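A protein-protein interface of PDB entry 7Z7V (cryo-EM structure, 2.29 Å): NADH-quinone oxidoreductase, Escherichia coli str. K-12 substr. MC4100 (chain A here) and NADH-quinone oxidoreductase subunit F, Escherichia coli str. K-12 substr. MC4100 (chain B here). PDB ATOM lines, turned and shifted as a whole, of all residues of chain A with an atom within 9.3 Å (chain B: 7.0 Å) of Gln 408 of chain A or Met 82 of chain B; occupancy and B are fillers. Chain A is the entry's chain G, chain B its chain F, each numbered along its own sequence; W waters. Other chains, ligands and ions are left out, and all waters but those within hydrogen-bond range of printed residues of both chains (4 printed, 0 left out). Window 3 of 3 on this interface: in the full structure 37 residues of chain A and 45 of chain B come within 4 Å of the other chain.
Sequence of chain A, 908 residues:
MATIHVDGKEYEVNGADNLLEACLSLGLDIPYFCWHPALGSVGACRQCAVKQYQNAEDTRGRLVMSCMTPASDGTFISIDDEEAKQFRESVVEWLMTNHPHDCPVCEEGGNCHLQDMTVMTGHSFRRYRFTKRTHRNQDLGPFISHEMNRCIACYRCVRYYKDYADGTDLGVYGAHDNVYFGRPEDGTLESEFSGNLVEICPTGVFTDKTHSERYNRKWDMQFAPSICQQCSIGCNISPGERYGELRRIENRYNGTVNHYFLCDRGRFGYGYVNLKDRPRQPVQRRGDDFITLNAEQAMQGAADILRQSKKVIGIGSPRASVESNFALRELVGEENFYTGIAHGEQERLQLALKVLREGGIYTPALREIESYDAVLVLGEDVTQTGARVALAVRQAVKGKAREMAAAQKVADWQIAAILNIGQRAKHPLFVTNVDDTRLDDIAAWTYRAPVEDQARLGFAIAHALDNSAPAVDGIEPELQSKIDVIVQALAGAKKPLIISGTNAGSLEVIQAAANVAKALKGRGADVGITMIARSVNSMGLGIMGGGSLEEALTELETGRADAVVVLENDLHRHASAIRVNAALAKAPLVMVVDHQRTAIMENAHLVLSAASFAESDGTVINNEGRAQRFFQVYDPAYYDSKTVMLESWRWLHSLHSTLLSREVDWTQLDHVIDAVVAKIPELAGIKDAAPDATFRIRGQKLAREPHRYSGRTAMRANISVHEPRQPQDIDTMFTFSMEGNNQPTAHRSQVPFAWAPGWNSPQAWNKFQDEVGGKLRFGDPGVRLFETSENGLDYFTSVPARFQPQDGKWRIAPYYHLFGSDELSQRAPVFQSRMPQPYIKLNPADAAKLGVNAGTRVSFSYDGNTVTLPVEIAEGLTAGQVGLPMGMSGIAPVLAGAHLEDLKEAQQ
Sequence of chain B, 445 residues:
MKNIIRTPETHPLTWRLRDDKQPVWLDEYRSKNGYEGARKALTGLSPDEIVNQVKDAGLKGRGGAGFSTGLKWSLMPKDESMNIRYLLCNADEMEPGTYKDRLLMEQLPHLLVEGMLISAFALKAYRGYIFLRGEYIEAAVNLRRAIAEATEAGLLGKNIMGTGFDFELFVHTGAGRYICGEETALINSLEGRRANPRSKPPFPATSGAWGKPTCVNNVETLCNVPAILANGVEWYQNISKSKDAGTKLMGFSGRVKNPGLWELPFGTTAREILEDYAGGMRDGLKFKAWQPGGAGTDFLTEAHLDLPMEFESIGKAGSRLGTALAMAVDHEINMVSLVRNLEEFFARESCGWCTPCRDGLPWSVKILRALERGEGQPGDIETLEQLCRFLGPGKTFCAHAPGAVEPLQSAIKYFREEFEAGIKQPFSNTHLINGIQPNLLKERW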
ATOM      1  N   ALA A 401      -9.785  27.534  28.181  1.00  0.00           N
ATOM      2  CA  ALA A 401      -8.883  26.818  27.288  1.00  0.00           C
ATOM      3  C   ALA A 401      -7.960  25.905  28.076  1.00  0.00           C
ATOM      4  O   ALA A 401      -7.657  24.789  27.633  1.00  0.00           O
ATOM      5  CB  ALA A 401      -8.068  27.804  26.454  1.00  0.00           C
ATOM      6  N   ARG A 402      -7.517  26.359  29.257  1.00  0.00           N
ATOM      7  CA  ARG A 402      -6.696  25.493  30.107  1.00  0.00           C
ATOM      8  C   ARG A 402      -7.438  24.216  30.501  1.00  0.00           C
ATOM      9  O   ARG A 402      -6.879  23.115  30.430  1.00  0.00           O
ATOM     10  CB  ARG A 402      -6.253  26.250  31.355  1.00  0.00           C
ATOM     11  CG  ARG A 402      -5.123  27.209  31.109  1.00  0.00           C
ATOM     12  CD  ARG A 402      -4.471  27.642  32.401  1.00  0.00           C
ATOM     13  NE  ARG A 402      -5.336  28.488  33.212  1.00  0.00           N
ATOM     14  CZ  ARG A 402      -5.500  29.791  33.034  1.00  0.00           C
ATOM     15  NH1 ARG A 402      -4.921  30.431  32.034  1.00  0.00           N
ATOM     16  NH2 ARG A 402      -6.262  30.470  33.886  1.00  0.00           N
ATOM     17  N   GLU A 403      -8.707  24.345  30.893  1.00  0.00           N
ATOM     18  CA  GLU A 403      -9.496  23.184  31.299  1.00  0.00           C
ATOM     19  C   GLU A 403      -9.789  22.255  30.122  1.00  0.00           C
ATOM     20  O   GLU A 403      -9.721  21.025  30.260  1.00  0.00           O
ATOM     21  CB  GLU A 403     -10.784  23.665  31.968  1.00  0.00           C
ATOM     22  CG  GLU A 403     -11.979  22.748  31.832  1.00  0.00           C
ATOM     23  CD  GLU A 403     -13.287  23.494  31.990  1.00  0.00           C
ATOM     24  OE1 GLU A 403     -13.350  24.405  32.843  1.00  0.00           O
ATOM     25  OE2 GLU A 403     -14.250  23.177  31.261  1.00  0.00           O
ATOM     26  N   MET A 404     -10.099  22.827  28.953  1.00  0.00           N
ATOM     27  CA  MET A 404     -10.354  22.018  27.764  1.00  0.00           C
ATOM     28  C   MET A 404      -9.115  21.237  27.348  1.00  0.00           C
ATOM     29  O   MET A 404      -9.215  20.079  26.932  1.00  0.00           O
ATOM     30  CB  MET A 404     -10.826  22.904  26.612  1.00  0.00           C
ATOM     31  CG  MET A 404     -12.260  23.373  26.725  1.00  0.00           C
ATOM     32  SD  MET A 404     -12.666  24.668  25.541  1.00  0.00           S
ATOM     33  CE  MET A 404     -11.854  24.062  24.072  1.00  0.00           C
ATOM     34  N   ALA A 405      -7.937  21.859  27.446  1.00  0.00           N
ATOM     35  CA  ALA A 405      -6.710  21.143  27.124  1.00  0.00           C
ATOM     36  C   ALA A 405      -6.372  20.095  28.175  1.00  0.00           C
ATOM     37  O   ALA A 405      -5.800  19.053  27.841  1.00  0.00           O
ATOM     38  CB  ALA A 405      -5.555  22.123  26.964  1.00  0.00           C
ATOM     39  N   ALA A 406      -6.703  20.352  29.444  1.00  0.00           N
ATOM     40  CA  ALA A 406      -6.496  19.341  30.473  1.00  0.00           C
ATOM     41  C   ALA A 406      -7.397  18.133  30.264  1.00  0.00           C
ATOM     42  O   ALA A 406      -7.023  17.014  30.633  1.00  0.00           O
ATOM     43  CB  ALA A 406      -6.731  19.937  31.860  1.00  0.00           C
ATOM     44  N   ALA A 407      -8.582  18.334  29.679  1.00  0.00           N
ATOM     45  CA  ALA A 407      -9.446  17.199  29.363  1.00  0.00           C
ATOM     46  C   ALA A 407      -8.850  16.310  28.276  1.00  0.00           C
ATOM     47  O   ALA A 407      -9.163  15.117  28.215  1.00  0.00           O
ATOM     48  CB  ALA A 407     -10.828  17.690  28.938  1.00  0.00           C
ATOM     49  N   GLN A 408      -7.989  16.862  27.420  1.00  0.00           N
ATOM     50  CA  GLN A 408      -7.387  16.121  26.320  1.00  0.00           C
ATOM     51  C   GLN A 408      -6.001  15.585  26.663  1.00  0.00           C
ATOM     52  O   GLN A 408      -5.243  15.236  25.753  1.00  0.00           O
ATOM     53  CB  GLN A 408      -7.317  17.002  25.074  1.00  0.00           C
ATOM     54  CG  GLN A 408      -8.617  17.078  24.301  1.00  0.00           C
ATOM     55  CD  GLN A 408      -8.435  17.661  22.918  1.00  0.00           C
ATOM     56  OE1 GLN A 408      -7.574  17.227  22.158  1.00  0.00           O
ATOM     57  NE2 GLN A 408      -9.253  18.648  22.582  1.00  0.00           N
ATOM     58  N   LYS A 409      -5.664  15.524  27.957  1.00  0.00           N
ATOM     59  CA  LYS A 409      -4.392  14.996  28.469  1.00  0.00           C
ATOM     60  C   LYS A 409      -3.186  15.765  27.933  1.00  0.00           C
ATOM     61  O   LYS A 409      -2.116  15.194  27.718  1.00  0.00           O
ATOM     62  CB  LYS A 409      -4.239  13.495  28.183  1.00  0.00           C
ATOM     63  CG  LYS A 409      -4.675  12.550  29.307  1.00  0.00           C
ATOM     64  CD  LYS A 409      -5.927  13.011  30.033  1.00  0.00           C
ATOM     65  CE  LYS A 409      -7.180  12.440  29.392  1.00  0.00           C
ATOM     66  NZ  LYS A 409      -8.401  12.748  30.185  1.00  0.00           N
ATOM     67  N   VAL A 410      -3.347  17.061  27.716  1.00  0.00           N
ATOM     68  CA  VAL A 410      -2.246  17.934  27.334  1.00  0.00           C
ATOM     69  C   VAL A 410      -1.646  18.520  28.604  1.00  0.00           C
ATOM     70  O   VAL A 410      -2.378  18.942  29.507  1.00  0.00           O
ATOM     71  CB  VAL A 410      -2.726  19.039  26.377  1.00  0.00           C
ATOM     72  CG1 VAL A 410      -1.602  19.999  26.039  1.00  0.00           C
ATOM     73  CG2 VAL A 410      -3.285  18.426  25.112  1.00  0.00           C
ATOM     74  N   ALA A 411      -0.317  18.513  28.689  1.00  0.00           N
ATOM     75  CA  ALA A 411       0.369  19.054  29.852  1.00  0.00           C
ATOM     76  C   ALA A 411       0.124  20.553  29.974  1.00  0.00           C
ATOM     77  O   ALA A 411      -0.056  21.259  28.980  1.00  0.00           O
ATOM     78  CB  ALA A 411       1.865  18.771  29.760  1.00  0.00           C
ATOM     79  N   GLN A 414       2.420  23.099  28.030  1.00  0.00           N
ATOM     80  CA  GLN A 414       2.452  23.091  26.567  1.00  0.00           C
ATOM     81  C   GLN A 414       1.449  24.123  26.062  1.00  0.00           C
ATOM     82  O   GLN A 414       0.359  23.800  25.587  1.00  0.00           O
ATOM     83  CB  GLN A 414       2.150  21.701  26.028  1.00  0.00           C
ATOM     84  CG  GLN A 414       3.261  21.125  25.181  1.00  0.00           C
ATOM     85  CD  GLN A 414       2.796  19.994  24.297  1.00  0.00           C
ATOM     86  OE1 GLN A 414       2.413  18.931  24.783  1.00  0.00           O
ATOM     87  NE2 GLN A 414       2.829  20.213  22.989  1.00  0.00           N
ATOM     88  N   ALA A 417      -0.281  24.188  22.416  1.00  0.00           N
ATOM     89  CA  ALA A 417      -1.336  23.193  22.266  1.00  0.00           C
ATOM     90  C   ALA A 417      -2.598  23.602  23.016  1.00  0.00           C
ATOM     91  O   ALA A 417      -3.713  23.381  22.529  1.00  0.00           O
ATOM     92  CB  ALA A 417      -0.842  21.832  22.748  1.00  0.00           C
ATOM     93  N   ILE A 418      -2.437  24.201  24.199  1.00  0.00           N
ATOM     94  CA  ILE A 418      -3.581  24.667  24.981  1.00  0.00           C
ATOM     95  C   ILE A 418      -4.324  25.769  24.236  1.00  0.00           C
ATOM     96  O   ILE A 418      -5.557  25.759  24.149  1.00  0.00           O
ATOM     97  CB  ILE A 418      -3.118  25.141  26.372  1.00  0.00           C
ATOM     98  CG1 ILE A 418      -2.460  23.993  27.137  1.00  0.00           C
ATOM     99  CG2 ILE A 418      -4.281  25.717  27.163  1.00  0.00           C
ATOM    100  CD1 ILE A 418      -1.805  24.409  28.420  1.00  0.00           C
ATOM    101  N   ASN A 420      -4.254  26.302  21.002  1.00  0.00           N
ATOM    102  CA  ASN A 420      -4.849  25.754  19.789  1.00  0.00           C
ATOM    103  C   ASN A 420      -6.140  25.008  20.092  1.00  0.00           C
ATOM    104  O   ASN A 420      -7.106  25.097  19.326  1.00  0.00           O
ATOM    105  CB  ASN A 420      -3.855  24.834  19.082  1.00  0.00           C
ATOM    106  CG  ASN A 420      -4.444  24.181  17.852  1.00  0.00           C
ATOM    107  OD1 ASN A 420      -4.849  24.858  16.913  1.00  0.00           O
ATOM    108  ND2 ASN A 420      -4.500  22.857  17.854  1.00  0.00           N
ATOM    109  N   ILE A 421      -6.173  24.258  21.195  1.00  0.00           N
ATOM    110  CA  ILE A 421      -7.391  23.547  21.580  1.00  0.00           C
ATOM    111  C   ILE A 421      -8.489  24.532  21.965  1.00  0.00           C
ATOM    112  O   ILE A 421      -9.646  24.382  21.556  1.00  0.00           O
ATOM    113  CB  ILE A 421      -7.079  22.555  22.716  1.00  0.00           C
ATOM    114  CG1 ILE A 421      -6.377  21.321  22.154  1.00  0.00           C
ATOM    115  CG2 ILE A 421      -8.339  22.147  23.463  1.00  0.00           C
ATOM    116  CD1 ILE A 421      -5.773  20.442  23.202  1.00  0.00           C
ATOM    117  N   GLY A 422      -8.140  25.565  22.732  1.00  0.00           N
ATOM    118  CA  GLY A 422      -9.144  26.492  23.225  1.00  0.00           C
ATOM    119  C   GLY A 422      -9.768  27.355  22.147  1.00  0.00           C
ATOM    120  O   GLY A 422     -10.975  27.610  22.176  1.00  0.00           O
ATOM    121  N   GLN A 423      -8.957  27.815  21.187  1.00  0.00           N
ATOM    122  CA  GLN A 423      -9.356  28.729  20.107  1.00  0.00           C
ATOM    123  C   GLN A 423      -9.886  30.008  20.741  1.00  0.00           C
ATOM    124  O   GLN A 423      -9.145  30.649  21.506  1.00  0.00           O
ATOM    125  CB  GLN A 423     -10.315  28.020  19.145  1.00  0.00           C
ATOM    126  CG  GLN A 423      -9.660  26.984  18.271  1.00  0.00           C
ATOM    127  CD  GLN A 423      -8.580  27.565  17.390  1.00  0.00           C
ATOM    128  OE1 GLN A 423      -8.826  28.478  16.610  1.00  0.00           O
ATOM    129  NE2 GLN A 423      -7.375  27.031  17.505  1.00  0.00           N
ATOM    130  N   PRO B  77      -9.781  10.682  17.000  1.00  0.00           N
ATOM    131  CA  PRO B  77     -10.444  10.213  18.221  1.00  0.00           C
ATOM    132  C   PRO B  77     -11.748   9.491  17.930  1.00  0.00           C
ATOM    133  O   PRO B  77     -12.445   9.777  16.955  1.00  0.00           O
ATOM    134  CB  PRO B  77     -10.695  11.504  19.011  1.00  0.00           C
ATOM    135  CG  PRO B  77      -9.835  12.535  18.374  1.00  0.00           C
ATOM    136  CD  PRO B  77      -9.729  12.150  16.944  1.00  0.00           C
ATOM    137  N   LYS B  78     -12.070   8.540  18.801  1.00  0.00           N
ATOM    138  CA  LYS B  78     -13.318   7.796  18.724  1.00  0.00           C
ATOM    139  C   LYS B  78     -14.458   8.498  19.444  1.00  0.00           C
ATOM    140  O   LYS B  78     -15.550   7.931  19.544  1.00  0.00           O
ATOM    141  CB  LYS B  78     -13.133   6.390  19.299  1.00  0.00           C
ATOM    142  CG  LYS B  78     -11.828   5.725  18.904  1.00  0.00           C
ATOM    143  CD  LYS B  78     -11.859   5.251  17.461  1.00  0.00           C
ATOM    144  CE  LYS B  78     -13.011   4.292  17.215  1.00  0.00           C
ATOM    145  NZ  LYS B  78     -13.282   4.111  15.763  1.00  0.00           N
ATOM    146  N   ASP B  79     -14.223   9.704  19.957  1.00  0.00           N
ATOM    147  CA  ASP B  79     -15.265  10.475  20.617  1.00  0.00           C
ATOM    148  C   ASP B  79     -16.341  10.875  19.615  1.00  0.00           C
ATOM    149  O   ASP B  79     -16.045  11.459  18.569  1.00  0.00           O
ATOM    150  CB  ASP B  79     -14.659  11.718  21.267  1.00  0.00           C
ATOM    151  CG  ASP B  79     -15.480  12.237  22.433  1.00  0.00           C
ATOM    152  OD1 ASP B  79     -16.725  12.149  22.386  1.00  0.00           O
ATOM    153  OD2 ASP B  79     -14.875  12.745  23.399  1.00  0.00           O
ATOM    154  N   GLU B  80     -17.593  10.560  19.940  1.00  0.00           N
ATOM    155  CA  GLU B  80     -18.711  10.926  19.081  1.00  0.00           C
ATOM    156  C   GLU B  80     -19.063  12.403  19.179  1.00  0.00           C
ATOM    157  O   GLU B  80     -19.687  12.939  18.257  1.00  0.00           O
ATOM    158  CB  GLU B  80     -19.939  10.082  19.428  1.00  0.00           C
ATOM    159  CG  GLU B  80     -19.761   8.594  19.180  1.00  0.00           C
ATOM    160  CD  GLU B  80     -19.651   8.257  17.708  1.00  0.00           C
ATOM    161  OE1 GLU B  80     -20.363   8.886  16.898  1.00  0.00           O
ATOM    162  OE2 GLU B  80     -18.853   7.362  17.360  1.00  0.00           O
ATOM    163  N   SER B  81     -18.678  13.070  20.267  1.00  0.00           N
ATOM    164  CA  SER B  81     -18.957  14.492  20.418  1.00  0.00           C
ATOM    165  C   SER B  81     -18.056  15.361  19.552  1.00  0.00           C
ATOM    166  O   SER B  81     -18.391  16.524  19.307  1.00  0.00           O
ATOM    167  CB  SER B  81     -18.814  14.905  21.883  1.00  0.00           C
ATOM    168  OG  SER B  81     -17.456  14.913  22.281  1.00  0.00           O
ATOM    169  N   MET B  82     -16.924  14.830  19.089  1.00  0.00           N
ATOM    170  CA  MET B  82     -16.038  15.549  18.176  1.00  0.00           C
ATOM    171  C   MET B  82     -16.515  15.288  16.750  1.00  0.00           C
ATOM    172  O   MET B  82     -15.954  14.485  16.004  1.00  0.00           O
ATOM    173  CB  MET B  82     -14.592  15.114  18.378  1.00  0.00           C
ATOM    174  CG  MET B  82     -13.991  15.545  19.701  1.00  0.00           C
ATOM    175  SD  MET B  82     -12.344  14.862  19.952  1.00  0.00           S
ATOM    176  CE  MET B  82     -11.785  15.822  21.354  1.00  0.00           C
ATOM    177  N   ASN B  83     -17.585  15.980  16.376  1.00  0.00           N
ATOM    178  CA  ASN B  83     -18.222  15.783  15.082  1.00  0.00           C
ATOM    179  C   ASN B  83     -17.728  16.747  14.012  1.00  0.00           C
ATOM    180  O   ASN B  83     -18.185  16.663  12.868  1.00  0.00           O
ATOM    181  CB  ASN B  83     -19.740  15.910  15.222  1.00  0.00           C
ATOM    182  CG  ASN B  83     -20.174  17.313  15.580  1.00  0.00           C
ATOM    183  OD1 ASN B  83     -19.656  17.915  16.519  1.00  0.00           O
ATOM    184  ND2 ASN B  83     -21.128  17.846  14.828  1.00  0.00           N
ATOM    185  N   ILE B  84     -16.820  17.657  14.347  1.00  0.00           N
ATOM    186  CA  ILE B  84     -16.270  18.611  13.393  1.00  0.00           C
ATOM    187  C   ILE B  84     -14.876  18.134  13.017  1.00  0.00           C
ATOM    188  O   ILE B  84     -13.980  18.085  13.867  1.00  0.00           O
ATOM    189  CB  ILE B  84     -16.236  20.031  13.980  1.00  0.00           C
ATOM    190  CG1 ILE B  84     -17.656  20.562  14.176  1.00  0.00           C
ATOM    191  CG2 ILE B  84     -15.425  20.961  13.097  1.00  0.00           C
ATOM    192  CD1 ILE B  84     -18.414  20.773  12.890  1.00  0.00           C
ATOM    193  N   ARG B  85     -14.685  17.772  11.750  1.00  0.00           N
ATOM    194  CA  ARG B  85     -13.425  17.182  11.328  1.00  0.00           C
ATOM    195  C   ARG B  85     -12.995  17.715   9.968  1.00  0.00           C
ATOM    196  O   ARG B  85     -13.819  18.041   9.093  1.00  0.00           O
ATOM    197  CB  ARG B  85     -13.508  15.653  11.301  1.00  0.00           C
ATOM    198  CG  ARG B  85     -13.259  15.011  12.646  1.00  0.00           C
ATOM    199  CD  ARG B  85     -13.868  13.629  12.736  1.00  0.00           C
ATOM    200  NE  ARG B  85     -14.156  13.256  14.114  1.00  0.00           N
ATOM    201  CZ  ARG B  85     -13.673  12.180  14.717  1.00  0.00           C
ATOM    202  NH1 ARG B  85     -12.874  11.335  14.088  1.00  0.00           N
ATOM    203  NH2 ARG B  85     -14.002  11.943  15.983  1.00  0.00           N
ATOM    204  N   LYS B 124     -14.696  10.755   8.466  1.00  0.00           N
ATOM    205  CA  LYS B 124     -15.886  11.496   8.888  1.00  0.00           C
ATOM    206  C   LYS B 124     -15.613  12.996   8.918  1.00  0.00           C
ATOM    207  O   LYS B 124     -16.078  13.717   9.801  1.00  0.00           O
ATOM    208  CB  LYS B 124     -16.412  11.001  10.238  1.00  0.00           C
ATOM    209  CG  LYS B 124     -16.807   9.538  10.241  1.00  0.00           C
ATOM    210  CD  LYS B 124     -17.213   9.075  11.624  1.00  0.00           C
ATOM    211  CE  LYS B 124     -16.001   8.719  12.465  1.00  0.00           C
ATOM    212  NZ  LYS B 124     -15.290   7.528  11.927  1.00  0.00           N
ATOM    213  N   PRO B 202       0.637  17.243  20.863  1.00  0.00           N
ATOM    214  CA  PRO B 202      -0.417  16.525  20.137  1.00  0.00           C
ATOM    215  C   PRO B 202      -0.297  16.603  18.621  1.00  0.00           C
ATOM    216  O   PRO B 202       0.093  17.623  18.062  1.00  0.00           O
ATOM    217  CB  PRO B 202      -1.694  17.220  20.609  1.00  0.00           C
ATOM    218  CG  PRO B 202      -1.268  18.583  20.926  1.00  0.00           C
ATOM    219  CD  PRO B 202       0.123  18.481  21.471  1.00  0.00           C
ATOM    220  N   ALA B 205      -4.180  14.790  14.246  1.00  0.00           N
ATOM    221  CA  ALA B 205      -5.309  13.870  14.307  1.00  0.00           C
ATOM    222  C   ALA B 205      -6.165  14.099  15.546  1.00  0.00           C
ATOM    223  O   ALA B 205      -7.381  13.893  15.501  1.00  0.00           O
ATOM    224  CB  ALA B 205      -4.810  12.426  14.270  1.00  0.00           C
ATOM    225  N   THR B 206      -5.563  14.533  16.651  1.00  0.00           N
ATOM    226  CA  THR B 206      -6.336  14.809  17.854  1.00  0.00           C
ATOM    227  C   THR B 206      -6.744  16.276  17.949  1.00  0.00           C
ATOM    228  O   THR B 206      -7.901  16.579  18.257  1.00  0.00           O
ATOM    229  CB  THR B 206      -5.551  14.392  19.101  1.00  0.00           C
ATOM    230  OG1 THR B 206      -4.190  14.821  18.983  1.00  0.00           O
ATOM    231  CG2 THR B 206      -5.579  12.884  19.252  1.00  0.00           C
ATOM    232  N   SER B 207      -5.819  17.197  17.685  1.00  0.00           N
ATOM    233  CA  SER B 207      -6.110  18.631  17.728  1.00  0.00           C
ATOM    234  C   SER B 207      -5.285  19.317  16.646  1.00  0.00           C
ATOM    235  O   SER B 207      -4.111  19.630  16.855  1.00  0.00           O
ATOM    236  CB  SER B 207      -5.819  19.215  19.105  1.00  0.00           C
ATOM    237  OG  SER B 207      -4.472  19.004  19.475  1.00  0.00           O
ATOM    238  N   GLY B 211      -8.144  23.454  16.424  1.00  0.00           N
ATOM    239  CA  GLY B 211      -8.298  22.546  17.536  1.00  0.00           C
ATOM    240  C   GLY B 211      -9.054  21.274  17.232  1.00  0.00           C
ATOM    241  O   GLY B 211      -9.121  20.394  18.098  1.00  0.00           O
ATOM    242  N   LYS B 212      -9.620  21.140  16.040  1.00  0.00           N
ATOM    243  CA  LYS B 212     -10.421  19.985  15.682  1.00  0.00           C
ATOM    244  C   LYS B 212      -9.539  18.850  15.183  1.00  0.00           C
ATOM    245  O   LYS B 212      -8.377  19.064  14.835  1.00  0.00           O
ATOM    246  CB  LYS B 212     -11.438  20.367  14.613  1.00  0.00           C
ATOM    247  CG  LYS B 212     -12.209  21.625  14.922  1.00  0.00           C
ATOM    248  CD  LYS B 212     -13.043  21.465  16.173  1.00  0.00           C
ATOM    249  CE  LYS B 212     -14.027  22.607  16.313  1.00  0.00           C
ATOM    250  NZ  LYS B 212     -13.340  23.928  16.302  1.00  0.00           N
ATOM    251  N   PRO B 213     -10.054  17.621  15.187  1.00  0.00           N
ATOM    252  CA  PRO B 213      -9.352  16.530  14.500  1.00  0.00           C
ATOM    253  C   PRO B 213      -9.165  16.823  13.017  1.00  0.00           C
ATOM    254  O   PRO B 213     -10.109  17.176  12.297  1.00  0.00           O
ATOM    255  CB  PRO B 213     -10.257  15.314  14.734  1.00  0.00           C
ATOM    256  CG  PRO B 213     -11.307  15.741  15.696  1.00  0.00           C
ATOM    257  CD  PRO B 213     -11.030  17.119  16.164  1.00  0.00           C
HETATM  258  O   HOH W   1      -3.399  21.419  20.174  1.00  0.00           O
HETATM  259  O   HOH W   2      -9.756  18.394  19.271  1.00  0.00           O
HETATM  260  O   HOH W   3     -10.912  22.106  20.292  1.00  0.00           O
HETATM  261  O   HOH W   4      -5.208  17.156  21.736  1.00  0.00           O
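The backbone carbonyl oxygen (O) of Ser 207 of chain B is in hydrogen-bond range of the side-chain amide nitrogen (ND2) of Asn 420 of chain A (3.4 Å).
The backbone NH of Gly 211 of chain B lies close to the backbone carbonyl oxygen of Asn 420 of chain A, at 3.5 Å.
Gln 408 of chain A touches Met 82 of chain B.
Gln 408 of chain A touches Thr 206 of chain B (OE1 to O, 3.97 Å).
Pro 202 of chain B touches Gln 414 of chain A.
CB of Ala 417 of chain A touches CD of Pro 202 of chain B (3.7 Å).
Ser 207 of chain B touches Ile 421 of chain A (CB to CG1, 3.7 Å).
Gly 211 of chain B touches Gln 423 of chain A (N to NE2, 3.8 Å).
Of the 18 printed residues of chain A, 6 touch a printed residue of chain B.
Hydrophobic or aromatic side chains of chain A that line the printed part of chain B: Ala 417 and Ile 421.
Along chain A the printed residues that touch a printed residue of chain B span positions 408 to 423.
Hydrophobic or aromatic side chains of chain B within 4 Å of the printed part of chain A: Met 82 and Pro 202.
Along chain B the printed residues that touch a printed residue of chain A span positions 82 to 211.
Among the printed residues, no Asp or Glu carboxylate lies within 4 Å of a Lys or Arg side-chain nitrogen of the other chain.
O of Met 82 of chain B sits at hydrogen-bond distance from NE of Arg 85 of chain B (2.9 Å).
The backbone carbonyl oxygen (O) of Asn 420 of chain A is in hydrogen-bond range of the side-chain amide nitrogen (NE2) of Gln 423 of chain A.
Water W4 lies within hydrogen-bond range of OE1 of Gln 408 of chain A (2.4 Å) and OG of Ser 207 of chain B (3.0 Å).
Water W2 lies within hydrogen-bond range of O of Gly 211 of chain B (2.4 Å), O of Thr 206 of chain B (2.8 Å) and NE2 of Gln 408 of chain A (3.4 Å).
Water W1 lies within hydrogen-bond range of the side-chain hydroxyl (OG) of Ser 207 of chain B, the side-chain amide nitrogen (ND2) of Asn 420 of chain A and the backbone carbonyl oxygen (O) of Ala 417 of chain A.
Water W3 lies within hydrogen-bond range of the backbone carbonyl oxygen of Ile 421 of chain A and the backbone carbonyl oxygen of Gly 211 of chain B.
Of the printed residues of chain B, Ile 421 of chain A touches Ser 207.
No residue of chain A comes within 4 Å of Ser 81 of chain B.
Printed residues of chain A within 4 Å of Met 82 of chain B: Gln 408.
Lys 124 of chain B touches none of the printed residues of chain A.
Of the printed residues of chain A, Ser 207 of chain B touches Asn 420 and Ile 421.
The nearest printed residue of chain B that does not touch Asn 420 of chain A is Lys 212 of chain B (5.7 Å).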
